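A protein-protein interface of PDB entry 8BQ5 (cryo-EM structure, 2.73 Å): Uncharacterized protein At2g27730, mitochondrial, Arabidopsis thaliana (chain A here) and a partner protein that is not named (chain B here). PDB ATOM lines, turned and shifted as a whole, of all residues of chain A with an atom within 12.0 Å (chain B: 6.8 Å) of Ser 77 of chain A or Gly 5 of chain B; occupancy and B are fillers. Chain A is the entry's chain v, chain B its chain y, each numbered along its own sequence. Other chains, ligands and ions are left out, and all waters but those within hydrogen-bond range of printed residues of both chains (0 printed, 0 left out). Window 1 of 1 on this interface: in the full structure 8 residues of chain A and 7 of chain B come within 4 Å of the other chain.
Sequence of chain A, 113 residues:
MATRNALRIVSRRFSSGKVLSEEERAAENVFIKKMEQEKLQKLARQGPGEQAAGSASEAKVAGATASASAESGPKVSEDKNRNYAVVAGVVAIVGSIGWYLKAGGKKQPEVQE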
ATOM      1  N   LYS A  75      10.242 -14.881   4.823  1.00  0.00           N
ATOM      2  CA  LYS A  75      11.268 -13.875   5.064  1.00  0.00           C
ATOM      3  C   LYS A  75      10.714 -12.465   4.864  1.00  0.00           C
ATOM      4  O   LYS A  75      11.039 -11.547   5.617  1.00  0.00           O
ATOM      5  CB  LYS A  75      12.470 -14.115   4.145  1.00  0.00           C
ATOM      6  CG  LYS A  75      13.311 -12.883   3.864  1.00  0.00           C
ATOM      7  CD  LYS A  75      14.580 -12.888   4.699  1.00  0.00           C
ATOM      8  CE  LYS A  75      15.304 -11.556   4.614  1.00  0.00           C
ATOM      9  NZ  LYS A  75      15.499 -10.942   5.957  1.00  0.00           N
ATOM     10  N   VAL A  76       9.865 -12.302   3.852  1.00  0.00           N
ATOM     11  CA  VAL A  76       9.291 -11.006   3.510  1.00  0.00           C
ATOM     12  C   VAL A  76       7.799 -11.175   3.251  1.00  0.00           C
ATOM     13  O   VAL A  76       7.362 -12.186   2.692  1.00  0.00           O
ATOM     14  CB  VAL A  76      10.002 -10.380   2.290  1.00  0.00           C
ATOM     15  CG1 VAL A  76       9.827 -11.248   1.056  1.00  0.00           C
ATOM     16  CG2 VAL A  76       9.499  -8.967   2.034  1.00  0.00           C
ATOM     17  N   SER A  77       7.014 -10.190   3.682  1.00  0.00           N
ATOM     18  CA  SER A  77       5.604 -10.118   3.320  1.00  0.00           C
ATOM     19  C   SER A  77       5.477  -9.435   1.962  1.00  0.00           C
ATOM     20  O   SER A  77       5.998  -8.333   1.765  1.00  0.00           O
ATOM     21  CB  SER A  77       4.816  -9.365   4.387  1.00  0.00           C
ATOM     22  OG  SER A  77       3.708  -8.688   3.821  1.00  0.00           O
ATOM     23  N   GLU A  78       4.785 -10.088   1.027  1.00  0.00           N
ATOM     24  CA  GLU A  78       4.803  -9.665  -0.367  1.00  0.00           C
ATOM     25  C   GLU A  78       3.583  -8.862  -0.797  1.00  0.00           C
ATOM     26  O   GLU A  78       3.646  -8.187  -1.830  1.00  0.00           O
ATOM     27  CB  GLU A  78       4.943 -10.887  -1.283  1.00  0.00           C
ATOM     28  CG  GLU A  78       5.976 -11.900  -0.809  1.00  0.00           C
ATOM     29  CD  GLU A  78       7.380 -11.563  -1.272  1.00  0.00           C
ATOM     30  OE1 GLU A  78       8.208 -12.492  -1.388  1.00  0.00           O
ATOM     31  OE2 GLU A  78       7.662 -10.372  -1.521  1.00  0.00           O
ATOM     32  N   ASP A  79       2.483  -8.911  -0.049  1.00  0.00           N
ATOM     33  CA  ASP A  79       1.268  -8.185  -0.423  1.00  0.00           C
ATOM     34  C   ASP A  79       1.496  -6.699  -0.174  1.00  0.00           C
ATOM     35  O   ASP A  79       1.460  -6.237   0.968  1.00  0.00           O
ATOM     36  CB  ASP A  79       0.071  -8.705   0.362  1.00  0.00           C
ATOM     37  CG  ASP A  79      -1.241  -8.486  -0.362  1.00  0.00           C
ATOM     38  OD1 ASP A  79      -2.108  -9.381  -0.304  1.00  0.00           O
ATOM     39  OD2 ASP A  79      -1.409  -7.414  -0.982  1.00  0.00           O
ATOM     40  N   LYS A  80       1.721  -5.939  -1.248  1.00  0.00           N
ATOM     41  CA  LYS A  80       2.097  -4.537  -1.083  1.00  0.00           C
ATOM     42  C   LYS A  80       0.917  -3.686  -0.629  1.00  0.00           C
ATOM     43  O   LYS A  80       1.089  -2.745   0.154  1.00  0.00           O
ATOM     44  CB  LYS A  80       2.697  -3.994  -2.381  1.00  0.00           C
ATOM     45  CG  LYS A  80       3.970  -4.722  -2.786  1.00  0.00           C
ATOM     46  CD  LYS A  80       4.574  -4.105  -4.039  1.00  0.00           C
ATOM     47  CE  LYS A  80       5.176  -2.736  -3.767  1.00  0.00           C
ATOM     48  NZ  LYS A  80       6.383  -2.839  -2.895  1.00  0.00           N
ATOM     49  N   ASN A  81      -0.290  -3.996  -1.109  1.00  0.00           N
ATOM     50  CA  ASN A  81      -1.472  -3.282  -0.635  1.00  0.00           C
ATOM     51  C   ASN A  81      -1.686  -3.512   0.854  1.00  0.00           C
ATOM     52  O   ASN A  81      -2.024  -2.580   1.594  1.00  0.00           O
ATOM     53  CB  ASN A  81      -2.706  -3.717  -1.423  1.00  0.00           C
ATOM     54  CG  ASN A  81      -2.780  -3.077  -2.791  1.00  0.00           C
ATOM     55  OD1 ASN A  81      -2.093  -2.097  -3.072  1.00  0.00           O
ATOM     56  ND2 ASN A  81      -3.625  -3.628  -3.651  1.00  0.00           N
ATOM     57  N   ARG A  82      -1.493  -4.750   1.310  1.00  0.00           N
ATOM     58  CA  ARG A  82      -1.620  -5.043   2.733  1.00  0.00           C
ATOM     59  C   ARG A  82      -0.557  -4.309   3.541  1.00  0.00           C
ATOM     60  O   ARG A  82      -0.832  -3.827   4.643  1.00  0.00           O
ATOM     61  CB  ARG A  82      -1.538  -6.552   2.966  1.00  0.00           C
ATOM     62  CG  ARG A  82      -1.835  -6.973   4.394  1.00  0.00           C
ATOM     63  CD  ARG A  82      -1.716  -8.478   4.563  1.00  0.00           C
ATOM     64  NE  ARG A  82      -0.348  -8.945   4.376  1.00  0.00           N
ATOM     65  CZ  ARG A  82      -0.003  -9.958   3.592  1.00  0.00           C
ATOM     66  NH1 ARG A  82      -0.903 -10.627   2.892  1.00  0.00           N
ATOM     67  NH2 ARG A  82       1.277 -10.305   3.509  1.00  0.00           N
ATOM     68  N   ASN A  83       0.663  -4.217   3.010  1.00  0.00           N
ATOM     69  CA  ASN A  83       1.715  -3.468   3.694  1.00  0.00           C
ATOM     70  C   ASN A  83       1.355  -1.992   3.812  1.00  0.00           C
ATOM     71  O   ASN A  83       1.544  -1.379   4.871  1.00  0.00           O
ATOM     72  CB  ASN A  83       3.037  -3.634   2.951  1.00  0.00           C
ATOM     73  CG  ASN A  83       3.483  -5.075   2.882  1.00  0.00           C
ATOM     74  OD1 ASN A  83       2.927  -5.940   3.559  1.00  0.00           O
ATOM     75  ND2 ASN A  83       4.489  -5.347   2.061  1.00  0.00           N
ATOM     76  N   TYR A  84       0.834  -1.408   2.731  1.00  0.00           N
ATOM     77  CA  TYR A  84       0.400  -0.016   2.776  1.00  0.00           C
ATOM     78  C   TYR A  84      -0.712   0.179   3.796  1.00  0.00           C
ATOM     79  O   TYR A  84      -0.724   1.172   4.530  1.00  0.00           O
ATOM     80  CB  TYR A  84      -0.071   0.438   1.397  1.00  0.00           C
ATOM     81  CG  TYR A  84       0.959   0.329   0.301  1.00  0.00           C
ATOM     82  CD1 TYR A  84       2.316   0.267   0.588  1.00  0.00           C
ATOM     83  CD2 TYR A  84       0.568   0.288  -1.026  1.00  0.00           C
ATOM     84  CE1 TYR A  84       3.251   0.170  -0.422  1.00  0.00           C
ATOM     85  CE2 TYR A  84       1.489   0.194  -2.035  1.00  0.00           C
ATOM     86  CZ  TYR A  84       2.825   0.134  -1.732  1.00  0.00           C
ATOM     87  OH  TYR A  84       3.726   0.044  -2.758  1.00  0.00           O
ATOM     88  N   ALA A  85      -1.662  -0.756   3.846  1.00  0.00           N
ATOM     89  CA  ALA A  85      -2.743  -0.658   4.821  1.00  0.00           C
ATOM     90  C   ALA A  85      -2.220  -0.780   6.247  1.00  0.00           C
ATOM     91  O   ALA A  85      -2.720  -0.116   7.161  1.00  0.00           O
ATOM     92  CB  ALA A  85      -3.796  -1.726   4.544  1.00  0.00           C
ATOM     93  N   VAL A  86      -1.226  -1.644   6.459  1.00  0.00           N
ATOM     94  CA  VAL A  86      -0.618  -1.774   7.780  1.00  0.00           C
ATOM     95  C   VAL A  86       0.041  -0.462   8.185  1.00  0.00           C
ATOM     96  O   VAL A  86      -0.111   0.004   9.323  1.00  0.00           O
ATOM     97  CB  VAL A  86       0.381  -2.947   7.788  1.00  0.00           C
ATOM     98  CG1 VAL A  86       1.308  -2.858   8.985  1.00  0.00           C
ATOM     99  CG2 VAL A  86      -0.364  -4.271   7.788  1.00  0.00           C
ATOM    100  N   VAL A  87       0.761   0.161   7.253  1.00  0.00           N
ATOM    101  CA  VAL A  87       1.383   1.453   7.530  1.00  0.00           C
ATOM    102  C   VAL A  87       0.323   2.507   7.828  1.00  0.00           C
ATOM    103  O   VAL A  87       0.501   3.349   8.713  1.00  0.00           O
ATOM    104  CB  VAL A  87       2.289   1.870   6.357  1.00  0.00           C
ATOM    105  CG1 VAL A  87       2.742   3.314   6.513  1.00  0.00           C
ATOM    106  CG2 VAL A  87       3.484   0.945   6.275  1.00  0.00           C
ATOM    107  N   MET B   1       6.679  -6.395  -0.179  1.00  0.00           N
ATOM    108  CA  MET B   1       8.045  -6.701  -0.584  1.00  0.00           C
ATOM    109  C   MET B   1       8.981  -5.551  -0.229  1.00  0.00           C
ATOM    110  O   MET B   1       8.535  -4.440   0.053  1.00  0.00           O
ATOM    111  CB  MET B   1       8.103  -7.002  -2.087  1.00  0.00           C
ATOM    112  CG  MET B   1       9.505  -7.243  -2.640  1.00  0.00           C
ATOM    113  SD  MET B   1       9.529  -7.650  -4.400  1.00  0.00           S
ATOM    114  CE  MET B   1       9.154  -6.054  -5.124  1.00  0.00           C
ATOM    115  N   GLY B   2      10.283  -5.825  -0.246  1.00  0.00           N
ATOM    116  CA  GLY B   2      11.270  -4.805   0.026  1.00  0.00           C
ATOM    117  C   GLY B   2      11.524  -4.603   1.508  1.00  0.00           C
ATOM    118  O   GLY B   2      11.277  -5.470   2.350  1.00  0.00           O
ATOM    119  N   THR B   3      12.042  -3.412   1.821  1.00  0.00           N
ATOM    120  CA  THR B   3      12.374  -3.085   3.204  1.00  0.00           C
ATOM    121  C   THR B   3      11.128  -3.061   4.081  1.00  0.00           C
ATOM    122  O   THR B   3      11.147  -3.551   5.218  1.00  0.00           O
ATOM    123  CB  THR B   3      13.096  -1.738   3.259  1.00  0.00           C
ATOM    124  OG1 THR B   3      14.340  -1.835   2.556  1.00  0.00           O
ATOM    125  CG2 THR B   3      13.373  -1.338   4.700  1.00  0.00           C
ATOM    126  N   LEU B   4      10.035  -2.495   3.567  1.00  0.00           N
ATOM    127  CA  LEU B   4       8.796  -2.433   4.335  1.00  0.00           C
ATOM    128  C   LEU B   4       8.241  -3.826   4.608  1.00  0.00           C
ATOM    129  O   LEU B   4       7.762  -4.109   5.715  1.00  0.00           O
ATOM    130  CB  LEU B   4       7.770  -1.581   3.590  1.00  0.00           C
ATOM    131  CG  LEU B   4       6.417  -1.431   4.278  1.00  0.00           C
ATOM    132  CD1 LEU B   4       6.614  -0.804   5.642  1.00  0.00           C
ATOM    133  CD2 LEU B   4       5.481  -0.593   3.425  1.00  0.00           C
ATOM    134  N   GLY B   5       8.292  -4.707   3.607  1.00  0.00           N
ATOM    135  CA  GLY B   5       7.832  -6.070   3.811  1.00  0.00           C
ATOM    136  C   GLY B   5       8.627  -6.795   4.879  1.00  0.00           C
ATOM    137  O   GLY B   5       8.060  -7.460   5.749  1.00  0.00           O
ATOM    138  N   ARG B   6       9.956  -6.665   4.833  1.00  0.00           N
ATOM    139  CA  ARG B   6      10.801  -7.294   5.845  1.00  0.00           C
ATOM    140  C   ARG B   6      10.530  -6.725   7.231  1.00  0.00           C
ATOM    141  O   ARG B   6      10.494  -7.470   8.220  1.00  0.00           O
ATOM    142  CB  ARG B   6      12.273  -7.117   5.485  1.00  0.00           C
ATOM    143  CG  ARG B   6      12.716  -7.866   4.254  1.00  0.00           C
ATOM    144  CD  ARG B   6      14.214  -8.091   4.300  1.00  0.00           C
ATOM    145  NE  ARG B   6      14.953  -6.836   4.231  1.00  0.00           N
ATOM    146  CZ  ARG B   6      15.030  -6.062   3.157  1.00  0.00           C
ATOM    147  NH1 ARG B   6      14.451  -6.401   2.017  1.00  0.00           N
ATOM    148  NH2 ARG B   6      15.714  -4.923   3.227  1.00  0.00           N
ATOM    149  N   ALA B   7      10.359  -5.405   7.329  1.00  0.00           N
ATOM    150  CA  ALA B   7      10.076  -4.799   8.625  1.00  0.00           C
ATOM    151  C   ALA B   7       8.765  -5.319   9.199  1.00  0.00           C
ATOM    152  O   ALA B   7       8.685  -5.657  10.388  1.00  0.00           O
ATOM    153  CB  ALA B   7      10.042  -3.276   8.498  1.00  0.00           C
ATOM    154  N   ILE B   8       7.726  -5.399   8.366  1.00  0.00           N
ATOM    155  CA  ILE B   8       6.439  -5.891   8.844  1.00  0.00           C
ATOM    156  C   ILE B   8       6.532  -7.368   9.208  1.00  0.00           C
ATOM    157  O   ILE B   8       5.898  -7.825  10.166  1.00  0.00           O
ATOM    158  CB  ILE B   8       5.345  -5.613   7.799  1.00  0.00           C
ATOM    159  CG1 ILE B   8       5.026  -4.117   7.762  1.00  0.00           C
ATOM    160  CG2 ILE B   8       4.087  -6.423   8.087  1.00  0.00           C
ATOM    161  CD1 ILE B   8       4.209  -3.691   6.573  1.00  0.00           C
ATOM    162  N   TYR B   9       7.338  -8.122   8.460  1.00  0.00           N
ATOM    163  CA  TYR B   9       7.552  -9.557   8.773  1.00  0.00           C
ATOM    164  C   TYR B   9       8.196  -9.683  10.161  1.00  0.00           C
ATOM    165  O   TYR B   9       7.719 -10.508  10.949  1.00  0.00           O
ATOM    166  CB  TYR B   9       8.377 -10.223   7.670  1.00  0.00           C
ATOM    167  CG  TYR B   9       8.363 -11.727   7.674  1.00  0.00           C
ATOM    168  CD1 TYR B   9       9.240 -12.449   8.466  1.00  0.00           C
ATOM    169  CD2 TYR B   9       7.486 -12.431   6.868  1.00  0.00           C
ATOM    170  CE1 TYR B   9       9.234 -13.833   8.472  1.00  0.00           C
ATOM    171  CE2 TYR B   9       7.466 -13.814   6.860  1.00  0.00           C
ATOM    172  CZ  TYR B   9       8.342 -14.517   7.667  1.00  0.00           C
ATOM    173  OH  TYR B   9       8.331 -15.880   7.661  1.00  0.00           O
ATOM    174  N   THR B  10       9.228  -8.883  10.452  1.00  0.00           N
ATOM    175  CA  THR B  10       9.889  -8.948  11.753  1.00  0.00           C
ATOM    176  C   THR B  10       8.941  -8.538  12.876  1.00  0.00           C
ATOM    177  O   THR B  10       8.922  -9.157  13.953  1.00  0.00           O
ATOM    178  CB  THR B  10      11.132  -8.059  11.746  1.00  0.00           C
ATOM    179  OG1 THR B  10      12.081  -8.575  10.805  1.00  0.00           O
ATOM    180  CG2 THR B  10      11.772  -8.026  13.116  1.00  0.00           C
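Ser 77 of chain A touches just these residues of chain B: Met 1, Gly 5 and Tyr 9. Of the printed residues of chain A, Leu 4 of chain B touches Asn 83 and Val 87. No residue of chain A comes within 4 Å of Ala 7 of chain B. Of chain A, only Asn 83 (3.8 Å) and Val 86 (3.9 Å) come within 4 Å of Ile 8 of chain B. Tyr 9 of chain B touches three residues of chain A. Of the printed residues of chain B, Asn 83 of chain A touches Met 1, Leu 4, Gly 5 and Ile 8. Of the printed residues of chain B, Lys 80 of chain A touches Met 1 (3.99 Å). Thr 10 of chain B touches none of the printed residues of chain A. Asp 79 of chain A touches none of the printed residues of chain B. The nearest residue of chain B that does not touch Ser 77 of chain A is Arg 6 of chain B (4.7 Å). The nearest residue of chain A that does not touch Gly 5 of chain B is Lys 75 of chain A (5.1 Å).
Hydrophobic or aromatic side chains of chain B within 4 Å of the printed part of chain A: Met 1, Leu 4, Ile 8 and Tyr 9. Hydrophobic or aromatic side chains of chain A within 4 Å of the printed part of chain B: Val 76, Val 86 and Val 87. Among the printed residues, 18 pairs touch across the chains.
The backbone NH (N) of Met 1 of chain B sits close to the side-chain amide nitrogen (ND2) of Asn 83 of chain A, 3.3 Å away. The backbone carbonyl oxygen (O) of Ser 77 of chain A sits at hydrogen-bond distance from the backbone NH (N) of Met 1 of chain B.
CD of Arg 6 of chain B touches NZ of Lys 75 of chain A (3.5 Å). Lys 75 of chain A touches Tyr 9 of chain B (O to CG, 3.4 Å). Met 1 of chain B touches Val 76 of chain A. Val 76 of chain A touches Gly 2 of chain B. Val 76 of chain A touches Gly 5 of chain B. CG2 of Val 76 of chain A touches N of Arg 6 of chain B, at 3.7 Å. Gly 5 of chain B touches Ser 77 of chain A. Ser 77 of chain A touches Tyr 9 of chain B (N to CD2, 3.9 Å). Glu 78 of chain A touches Met 1 of chain B. Met 1 of chain B touches Lys 80 of chain A.
The side-chain hydroxyl (OG) of Ser 77 of chain A sits at hydrogen-bond distance from the guanidinium group (NH2) of Arg 82 of chain A (2.9 Å). The side-chain hydroxyl (OG1) of Thr 10 of chain B is in hydrogen-bond range of the backbone carbonyl oxygen (O) of Arg 6 of chain B (3.2 Å). The guanidinium group (NH1) of Arg 6 of chain B is in hydrogen-bond range of the backbone carbonyl oxygen (O) of Gly 2 of chain B. The backbone carbonyl oxygen of Asp 79 of chain A lies close to the side-chain amide oxygen of Asn 83 of chain A, at 3.0 Å. OG1 of Thr 3 of chain B sits at hydrogen-bond distance from NH2 of Arg 6 of chain B, at 3.4 Å. OG of Ser 77 of chain A lies within hydrogen-bond range of OD1 of Asn 83 of chain A.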
